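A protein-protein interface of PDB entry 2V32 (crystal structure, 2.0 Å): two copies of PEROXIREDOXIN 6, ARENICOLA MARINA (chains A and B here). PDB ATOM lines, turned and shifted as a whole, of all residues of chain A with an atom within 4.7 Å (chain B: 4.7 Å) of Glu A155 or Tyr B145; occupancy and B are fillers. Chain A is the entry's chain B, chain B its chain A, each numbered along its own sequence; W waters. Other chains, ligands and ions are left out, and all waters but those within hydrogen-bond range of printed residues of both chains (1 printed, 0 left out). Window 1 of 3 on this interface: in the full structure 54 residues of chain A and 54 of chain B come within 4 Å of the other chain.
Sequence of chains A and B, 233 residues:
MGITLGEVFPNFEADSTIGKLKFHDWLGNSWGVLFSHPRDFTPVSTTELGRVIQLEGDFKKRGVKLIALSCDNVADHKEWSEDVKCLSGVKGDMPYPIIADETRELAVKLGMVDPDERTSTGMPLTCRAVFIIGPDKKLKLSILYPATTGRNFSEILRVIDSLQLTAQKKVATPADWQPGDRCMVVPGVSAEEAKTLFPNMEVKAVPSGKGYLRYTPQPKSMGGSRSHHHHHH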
ATOM      1  N   LEU A   5      -3.038 -37.056 -19.024  1.00  0.00           N
ATOM      2  CA  LEU A   5      -2.531 -36.522 -17.756  1.00  0.00           C
ATOM      3  C   LEU A   5      -3.199 -37.175 -16.513  1.00  0.00           C
ATOM      4  O   LEU A   5      -4.400 -37.434 -16.493  1.00  0.00           O
ATOM      5  CB  LEU A   5      -2.630 -34.981 -17.725  1.00  0.00           C
ATOM      6  CG  LEU A   5      -1.911 -34.212 -18.850  1.00  0.00           C
ATOM      7  CD1 LEU A   5      -1.855 -32.756 -18.535  1.00  0.00           C
ATOM      8  CD2 LEU A   5      -0.441 -34.744 -19.212  1.00  0.00           C
ATOM      9  N   LEU A 141       2.953 -34.422 -17.728  1.00  0.00           N
ATOM     10  CA  LEU A 141       3.113 -33.596 -18.940  1.00  0.00           C
ATOM     11  C   LEU A 141       3.511 -34.516 -20.111  1.00  0.00           C
ATOM     12  O   LEU A 141       4.278 -35.480 -19.957  1.00  0.00           O
ATOM     13  CB  LEU A 141       4.183 -32.523 -18.683  1.00  0.00           C
ATOM     14  CG  LEU A 141       4.346 -31.351 -19.651  1.00  0.00           C
ATOM     15  CD1 LEU A 141       4.880 -30.235 -18.860  1.00  0.00           C
ATOM     16  CD2 LEU A 141       5.362 -31.805 -20.766  1.00  0.00           C
ATOM     17  N   ILE A 143       4.524 -34.438 -24.601  1.00  0.00           N
ATOM     18  CA  ILE A 143       4.630 -33.783 -25.935  1.00  0.00           C
ATOM     19  C   ILE A 143       4.761 -34.845 -27.009  1.00  0.00           C
ATOM     20  O   ILE A 143       5.436 -35.857 -26.797  1.00  0.00           O
ATOM     21  CB  ILE A 143       5.823 -32.803 -26.066  1.00  0.00           C
ATOM     22  CG1 ILE A 143       7.164 -33.560 -26.130  1.00  0.00           C
ATOM     23  CG2 ILE A 143       5.785 -31.682 -24.992  1.00  0.00           C
ATOM     24  CD1 ILE A 143       8.398 -32.673 -26.409  1.00  0.00           C
ATOM     25  N   ASN A 152      13.305 -29.506 -28.122  1.00  0.00           N
ATOM     26  CA  ASN A 152      13.921 -28.454 -27.365  1.00  0.00           C
ATOM     27  C   ASN A 152      14.063 -28.942 -25.922  1.00  0.00           C
ATOM     28  O   ASN A 152      13.080 -28.952 -25.147  1.00  0.00           O
ATOM     29  CB  ASN A 152      13.038 -27.195 -27.486  1.00  0.00           C
ATOM     30  CG  ASN A 152      13.523 -26.026 -26.624  1.00  0.00           C
ATOM     31  OD1 ASN A 152      14.417 -26.185 -25.784  1.00  0.00           O
ATOM     32  ND2 ASN A 152      12.880 -24.853 -26.793  1.00  0.00           N
ATOM     33  N   PHE A 153      15.253 -29.431 -25.585  1.00  0.00           N
ATOM     34  CA  PHE A 153      15.454 -30.017 -24.256  1.00  0.00           C
ATOM     35  C   PHE A 153      15.611 -28.986 -23.094  1.00  0.00           C
ATOM     36  O   PHE A 153      15.568 -29.341 -21.876  1.00  0.00           O
ATOM     37  CB  PHE A 153      16.548 -31.136 -24.272  1.00  0.00           C
ATOM     38  CG  PHE A 153      16.036 -32.468 -24.833  1.00  0.00           C
ATOM     39  CD1 PHE A 153      15.277 -33.316 -24.036  1.00  0.00           C
ATOM     40  CD2 PHE A 153      16.239 -32.803 -26.180  1.00  0.00           C
ATOM     41  CE1 PHE A 153      14.776 -34.534 -24.530  1.00  0.00           C
ATOM     42  CE2 PHE A 153      15.734 -33.998 -26.710  1.00  0.00           C
ATOM     43  CZ  PHE A 153      15.017 -34.870 -25.883  1.00  0.00           C
ATOM     44  N   SER A 154      15.782 -27.722 -23.458  1.00  0.00           N
ATOM     45  CA  SER A 154      15.762 -26.650 -22.477  1.00  0.00           C
ATOM     46  C   SER A 154      14.315 -26.472 -22.001  1.00  0.00           C
ATOM     47  O   SER A 154      14.052 -26.368 -20.808  1.00  0.00           O
ATOM     48  CB  SER A 154      16.264 -25.363 -23.120  1.00  0.00           C
ATOM     49  OG  SER A 154      17.659 -25.460 -23.435  1.00  0.00           O
ATOM     50  N   GLU A 155      13.353 -26.490 -22.920  1.00  0.00           N
ATOM     51  CA  GLU A 155      11.947 -26.436 -22.524  1.00  0.00           C
ATOM     52  C   GLU A 155      11.591 -27.593 -21.614  1.00  0.00           C
ATOM     53  O   GLU A 155      10.834 -27.405 -20.710  1.00  0.00           O
ATOM     54  CB  GLU A 155      11.022 -26.454 -23.750  1.00  0.00           C
ATOM     55  CG  GLU A 155       9.540 -26.478 -23.334  1.00  0.00           C
ATOM     56  CD  GLU A 155       9.037 -25.167 -22.776  1.00  0.00           C
ATOM     57  OE1 GLU A 155       9.800 -24.179 -22.822  1.00  0.00           O
ATOM     58  OE2 GLU A 155       7.832 -25.125 -22.355  1.00  0.00           O
ATOM     59  N   ILE A 156      12.115 -28.798 -21.851  1.00  0.00           N
ATOM     60  CA  ILE A 156      11.816 -29.942 -20.985  1.00  0.00           C
ATOM     61  C   ILE A 156      12.300 -29.618 -19.600  1.00  0.00           C
ATOM     62  O   ILE A 156      11.553 -29.771 -18.664  1.00  0.00           O
ATOM     63  CB  ILE A 156      12.417 -31.287 -21.510  1.00  0.00           C
ATOM     64  CG1 ILE A 156      11.669 -31.703 -22.760  1.00  0.00           C
ATOM     65  CG2 ILE A 156      12.286 -32.438 -20.480  1.00  0.00           C
ATOM     66  CD1 ILE A 156      12.591 -32.090 -23.860  1.00  0.00           C
ATOM     67  N   LEU A 157      13.534 -29.123 -19.485  1.00  0.00           N
ATOM     68  CA  LEU A 157      14.071 -28.614 -18.204  1.00  0.00           C
ATOM     69  C   LEU A 157      13.201 -27.560 -17.523  1.00  0.00           C
ATOM     70  O   LEU A 157      12.920 -27.672 -16.322  1.00  0.00           O
ATOM     71  CB  LEU A 157      15.506 -28.097 -18.384  1.00  0.00           C
ATOM     72  CG  LEU A 157      16.569 -29.191 -18.556  1.00  0.00           C
ATOM     73  CD1 LEU A 157      17.875 -28.608 -19.008  1.00  0.00           C
ATOM     74  CD2 LEU A 157      16.792 -29.975 -17.245  1.00  0.00           C
ATOM     75  N   ARG A 158      12.805 -26.538 -18.290  1.00  0.00           N
ATOM     76  CA  ARG A 158      11.954 -25.432 -17.796  1.00  0.00           C
ATOM     77  C   ARG A 158      10.660 -25.980 -17.191  1.00  0.00           C
ATOM     78  O   ARG A 158      10.313 -25.646 -16.029  1.00  0.00           O
ATOM     79  CB  ARG A 158      11.669 -24.433 -18.927  1.00  0.00           C
ATOM     80  CG  ARG A 158      10.892 -23.211 -18.461  1.00  0.00           C
ATOM     81  CD  ARG A 158      10.459 -22.421 -19.652  1.00  0.00           C
ATOM     82  NE  ARG A 158       9.255 -22.953 -20.240  1.00  0.00           N
ATOM     83  CZ  ARG A 158       8.021 -22.806 -19.764  1.00  0.00           C
ATOM     84  NH1 ARG A 158       7.775 -22.079 -18.687  1.00  0.00           N
ATOM     85  NH2 ARG A 158       7.006 -23.391 -20.405  1.00  0.00           N
ATOM     86  N   VAL A 159       9.939 -26.819 -17.954  1.00  0.00           N
ATOM     87  CA  VAL A 159       8.672 -27.381 -17.460  1.00  0.00           C
ATOM     88  C   VAL A 159       8.891 -28.313 -16.260  1.00  0.00           C
ATOM     89  O   VAL A 159       8.046 -28.370 -15.407  1.00  0.00           O
ATOM     90  CB  VAL A 159       7.807 -28.032 -18.580  1.00  0.00           C
ATOM     91  CG1 VAL A 159       7.454 -27.030 -19.545  1.00  0.00           C
ATOM     92  CG2 VAL A 159       8.523 -29.253 -19.270  1.00  0.00           C
ATOM     93  N   CYS B 127      -6.901 -29.072 -19.752  1.00  0.00           N
ATOM     94  CA  CYS B 127      -5.550 -28.705 -19.303  1.00  0.00           C
ATOM     95  C   CYS B 127      -5.074 -27.593 -20.252  1.00  0.00           C
ATOM     96  O   CYS B 127      -5.908 -26.893 -20.810  1.00  0.00           O
ATOM     97  CB  CYS B 127      -4.633 -29.954 -19.287  1.00  0.00           C
ATOM     98  SG  CYS B 127      -4.297 -30.668 -20.944  1.00  0.00           S
ATOM     99  N   ARG B 128      -3.769 -27.371 -20.392  1.00  0.00           N
ATOM    100  CA  ARG B 128      -3.214 -26.427 -21.373  1.00  0.00           C
ATOM    101  C   ARG B 128      -2.676 -27.258 -22.553  1.00  0.00           C
ATOM    102  O   ARG B 128      -1.477 -27.577 -22.643  1.00  0.00           O
ATOM    103  CB  ARG B 128      -2.101 -25.561 -20.778  1.00  0.00           C
ATOM    104  CG  ARG B 128      -2.436 -25.031 -19.418  1.00  0.00           C
ATOM    105  CD  ARG B 128      -1.545 -23.923 -18.923  1.00  0.00           C
ATOM    106  NE  ARG B 128      -2.020 -23.622 -17.591  1.00  0.00           N
ATOM    107  CZ  ARG B 128      -2.994 -22.780 -17.298  1.00  0.00           C
ATOM    108  NH1 ARG B 128      -3.571 -22.020 -18.235  1.00  0.00           N
ATOM    109  NH2 ARG B 128      -3.340 -22.676 -16.040  1.00  0.00           N
ATOM    110  N   ALA B 129      -3.598 -27.623 -23.433  1.00  0.00           N
ATOM    111  CA  ALA B 129      -3.289 -28.439 -24.594  1.00  0.00           C
ATOM    112  C   ALA B 129      -2.920 -27.534 -25.751  1.00  0.00           C
ATOM    113  O   ALA B 129      -3.390 -26.376 -25.835  1.00  0.00           O
ATOM    114  CB  ALA B 129      -4.483 -29.229 -24.938  1.00  0.00           C
ATOM    115  N   ILE B 143       0.978 -31.002 -27.511  1.00  0.00           N
ATOM    116  CA  ILE B 143       1.551 -30.975 -26.183  1.00  0.00           C
ATOM    117  C   ILE B 143       0.385 -30.915 -25.244  1.00  0.00           C
ATOM    118  O   ILE B 143      -0.658 -30.350 -25.582  1.00  0.00           O
ATOM    119  CB  ILE B 143       2.492 -29.736 -25.984  1.00  0.00           C
ATOM    120  CG1 ILE B 143       1.697 -28.496 -25.634  1.00  0.00           C
ATOM    121  CG2 ILE B 143       3.416 -29.523 -27.209  1.00  0.00           C
ATOM    122  CD1 ILE B 143       2.432 -27.204 -25.737  1.00  0.00           C
ATOM    123  N   LEU B 144       0.509 -31.598 -24.119  1.00  0.00           N
ATOM    124  CA  LEU B 144      -0.482 -31.515 -23.074  1.00  0.00           C
ATOM    125  C   LEU B 144       0.283 -31.079 -21.817  1.00  0.00           C
ATOM    126  O   LEU B 144       1.096 -31.859 -21.275  1.00  0.00           O
ATOM    127  CB  LEU B 144      -1.192 -32.849 -22.812  1.00  0.00           C
ATOM    128  CG  LEU B 144      -1.990 -33.615 -23.841  1.00  0.00           C
ATOM    129  CD1 LEU B 144      -2.434 -34.879 -23.108  1.00  0.00           C
ATOM    130  CD2 LEU B 144      -3.161 -32.778 -24.307  1.00  0.00           C
ATOM    131  N   TYR B 145       0.036 -29.843 -21.390  1.00  0.00           N
ATOM    132  CA  TYR B 145       0.645 -29.330 -20.185  1.00  0.00           C
ATOM    133  C   TYR B 145      -0.474 -29.231 -19.180  1.00  0.00           C
ATOM    134  O   TYR B 145      -1.579 -28.884 -19.572  1.00  0.00           O
ATOM    135  CB  TYR B 145       1.212 -27.906 -20.439  1.00  0.00           C
ATOM    136  CG  TYR B 145       2.568 -27.797 -21.086  1.00  0.00           C
ATOM    137  CD1 TYR B 145       3.075 -28.818 -21.878  1.00  0.00           C
ATOM    138  CD2 TYR B 145       3.341 -26.623 -20.939  1.00  0.00           C
ATOM    139  CE1 TYR B 145       4.291 -28.697 -22.467  1.00  0.00           C
ATOM    140  CE2 TYR B 145       4.555 -26.488 -21.535  1.00  0.00           C
ATOM    141  CZ  TYR B 145       5.034 -27.525 -22.309  1.00  0.00           C
ATOM    142  OH  TYR B 145       6.262 -27.448 -22.899  1.00  0.00           O
ATOM    143  N   PRO B 146      -0.188 -29.497 -17.883  1.00  0.00           N
ATOM    144  CA  PRO B 146      -1.151 -29.327 -16.802  1.00  0.00           C
ATOM    145  C   PRO B 146      -1.445 -27.835 -16.498  1.00  0.00           C
ATOM    146  O   PRO B 146      -0.746 -26.932 -17.040  1.00  0.00           O
ATOM    147  CB  PRO B 146      -0.450 -30.019 -15.602  1.00  0.00           C
ATOM    148  CG  PRO B 146       1.012 -29.774 -15.866  1.00  0.00           C
ATOM    149  CD  PRO B 146       1.124 -29.960 -17.373  1.00  0.00           C
ATOM    150  N   ALA B 147      -2.428 -27.603 -15.612  1.00  0.00           N
ATOM    151  CA  ALA B 147      -2.920 -26.260 -15.252  1.00  0.00           C
ATOM    152  C   ALA B 147      -1.870 -25.490 -14.504  1.00  0.00           C
ATOM    153  O   ALA B 147      -1.847 -24.241 -14.548  1.00  0.00           O
ATOM    154  CB  ALA B 147      -4.237 -26.350 -14.423  1.00  0.00           C
ATOM    155  N   THR B 149       1.227 -25.246 -15.093  1.00  0.00           N
ATOM    156  CA  THR B 149       2.384 -24.947 -15.881  1.00  0.00           C
ATOM    157  C   THR B 149       2.061 -24.236 -17.173  1.00  0.00           C
ATOM    158  O   THR B 149       1.706 -24.845 -18.156  1.00  0.00           O
ATOM    159  CB  THR B 149       3.192 -26.233 -16.119  1.00  0.00           C
ATOM    160  OG1 THR B 149       3.546 -26.784 -14.850  1.00  0.00           O
ATOM    161  CG2 THR B 149       4.424 -25.975 -16.985  1.00  0.00           C
ATOM    162  N   GLY B 150       2.175 -22.913 -17.139  1.00  0.00           N
ATOM    163  CA  GLY B 150       2.094 -22.102 -18.333  1.00  0.00           C
ATOM    164  C   GLY B 150       3.033 -22.511 -19.451  1.00  0.00           C
ATOM    165  O   GLY B 150       4.140 -22.995 -19.250  1.00  0.00           O
ATOM    166  N   ARG B 151       2.566 -22.272 -20.656  1.00  0.00           N
ATOM    167  CA  ARG B 151       3.224 -22.698 -21.884  1.00  0.00           C
ATOM    168  C   ARG B 151       4.355 -21.729 -22.335  1.00  0.00           C
ATOM    169  O   ARG B 151       4.473 -20.608 -21.870  1.00  0.00           O
ATOM    170  CB  ARG B 151       2.154 -22.865 -23.012  1.00  0.00           C
ATOM    171  CG  ARG B 151       1.367 -24.193 -22.922  1.00  0.00           C
ATOM    172  CD  ARG B 151       0.040 -24.163 -23.604  1.00  0.00           C
ATOM    173  NE  ARG B 151      -0.937 -23.193 -23.022  1.00  0.00           N
ATOM    174  CZ  ARG B 151      -2.255 -23.236 -23.254  1.00  0.00           C
ATOM    175  NH1 ARG B 151      -2.758 -24.155 -24.079  1.00  0.00           N
ATOM    176  NH2 ARG B 151      -3.087 -22.342 -22.703  1.00  0.00           N
ATOM    177  N   ASN B 152       5.219 -22.203 -23.230  1.00  0.00           N
ATOM    178  CA  ASN B 152       6.207 -21.356 -23.885  1.00  0.00           C
ATOM    179  C   ASN B 152       5.735 -21.173 -25.332  1.00  0.00           C
ATOM    180  O   ASN B 152       5.885 -22.073 -26.138  1.00  0.00           O
ATOM    181  CB  ASN B 152       7.526 -22.134 -23.807  1.00  0.00           C
ATOM    182  CG  ASN B 152       8.656 -21.471 -24.529  1.00  0.00           C
ATOM    183  OD1 ASN B 152       8.512 -20.413 -25.123  1.00  0.00           O
ATOM    184  ND2 ASN B 152       9.811 -22.073 -24.434  1.00  0.00           N
HETATM  185  O   HOH W   1       5.306 -21.607 -17.112  1.00  0.00           O
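Ile A143 touches its own counterpart, Ile B143.
2 positions are printed for both chains.
Of the 12 pairs that touch across the chains among the printed residues, 1 has its exchanged pair printed and touching as well.
Water W1 lies within hydrogen-bond range of O of Gly B150 and NH1 of Arg A158.
Printed residues of chain B within 4 Å of Leu A5: Leu B144 (3.9 Å), Tyr B145 (3.8 Å) and Pro B146 (3.7 Å).
Of chain B, only Tyr B145 (2.9 Å) and Asn B152 (2.7 Å) come within 4 Å of Glu A155.
Of the printed residues of chain B, Arg A158 touches Gly B150 (3.1 Å), Arg B151 (3.7 Å) and Asn B152 (3.5 Å).
Printed residues of chain A within 4 Å of Leu B144: Leu A5 (3.9 Å) and Leu A141 (3.5 Å).
Of chain A, only Leu A5 (3.8 Å), Leu A141 (3.6 Å), Glu A155 (2.9 Å) and Val A159 (3.6 Å) come within 4 Å of Tyr B145.
Of the printed residues of chain A, Pro B146 touches Leu A5.
Thr B149 touches none of the printed residues of chain A.
Printed residues of chain A within 4 Å of Arg B151: Arg A158.
Hydrophobic or aromatic side chains of chain B that line the printed part of chain A: Ile B143 and Tyr B145.
Along chain B the printed residues that touch a printed residue of chain A span positions 143 to 152.
Printed residues of chain A that touch a printed residue of chain B: Leu A5, Leu A141, Ile A143, Glu A155, Arg A158 and Val A159.
Along chain A the printed residues that touch a printed residue of chain B span positions 5 to 159.
Among the printed residues, no Asp or Glu carboxylate lies within 4 Å of a Lys or Arg side-chain nitrogen of the other chain.
Leu B144 touches Leu A5 (O to CD2, 3.9 Å).
Leu A5 touches Tyr B145.
Pro B146 touches Leu A5 (N to CD1, 3.7 Å).
Leu B144 touches Leu A141.
Leu A141 touches Tyr B145.
CG2 of Ile A143 touches CG2 of Ile B143, 3.9 Å away.
NH2 of Arg A158 touches C of Arg B151 (3.7 Å).
N of Asn B152 touches NH2 of Arg A158, 3.5 Å away.
Tyr B145 touches Val A159.
The side-chain hydroxyl (OH) of Tyr B145 is in hydrogen-bond range of the side-chain carboxylate (OE2) of Glu A155, at 2.9 Å.
The guanidinium group (NH2) of Arg A158 lies within hydrogen-bond range of the backbone carbonyl oxygen (O) of Gly B150.
The side-chain carboxylate of Glu A155 sits at hydrogen-bond distance from the side-chain amide nitrogen of Asn B152, 2.7 Å away.
SG of Cys B127 lies close to O of Tyr B145, 3.5 Å away.
The backbone NH (N) of Arg B128 lies within hydrogen-bond range of the backbone carbonyl oxygen (O) of Tyr B145, 2.8 Å away.
The backbone carbonyl oxygen of Ala B129 lies within hydrogen-bond range of the guanidinium group of Arg B151, 2.9 Å away.
The side-chain amide oxygen (OD1) of Asn A152 sits at hydrogen-bond distance from the backbone NH (N) of Glu A155.
OE2 of Glu A155 lies within salt-bridge range of NH2 of Arg A158, 2.7 Å away.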
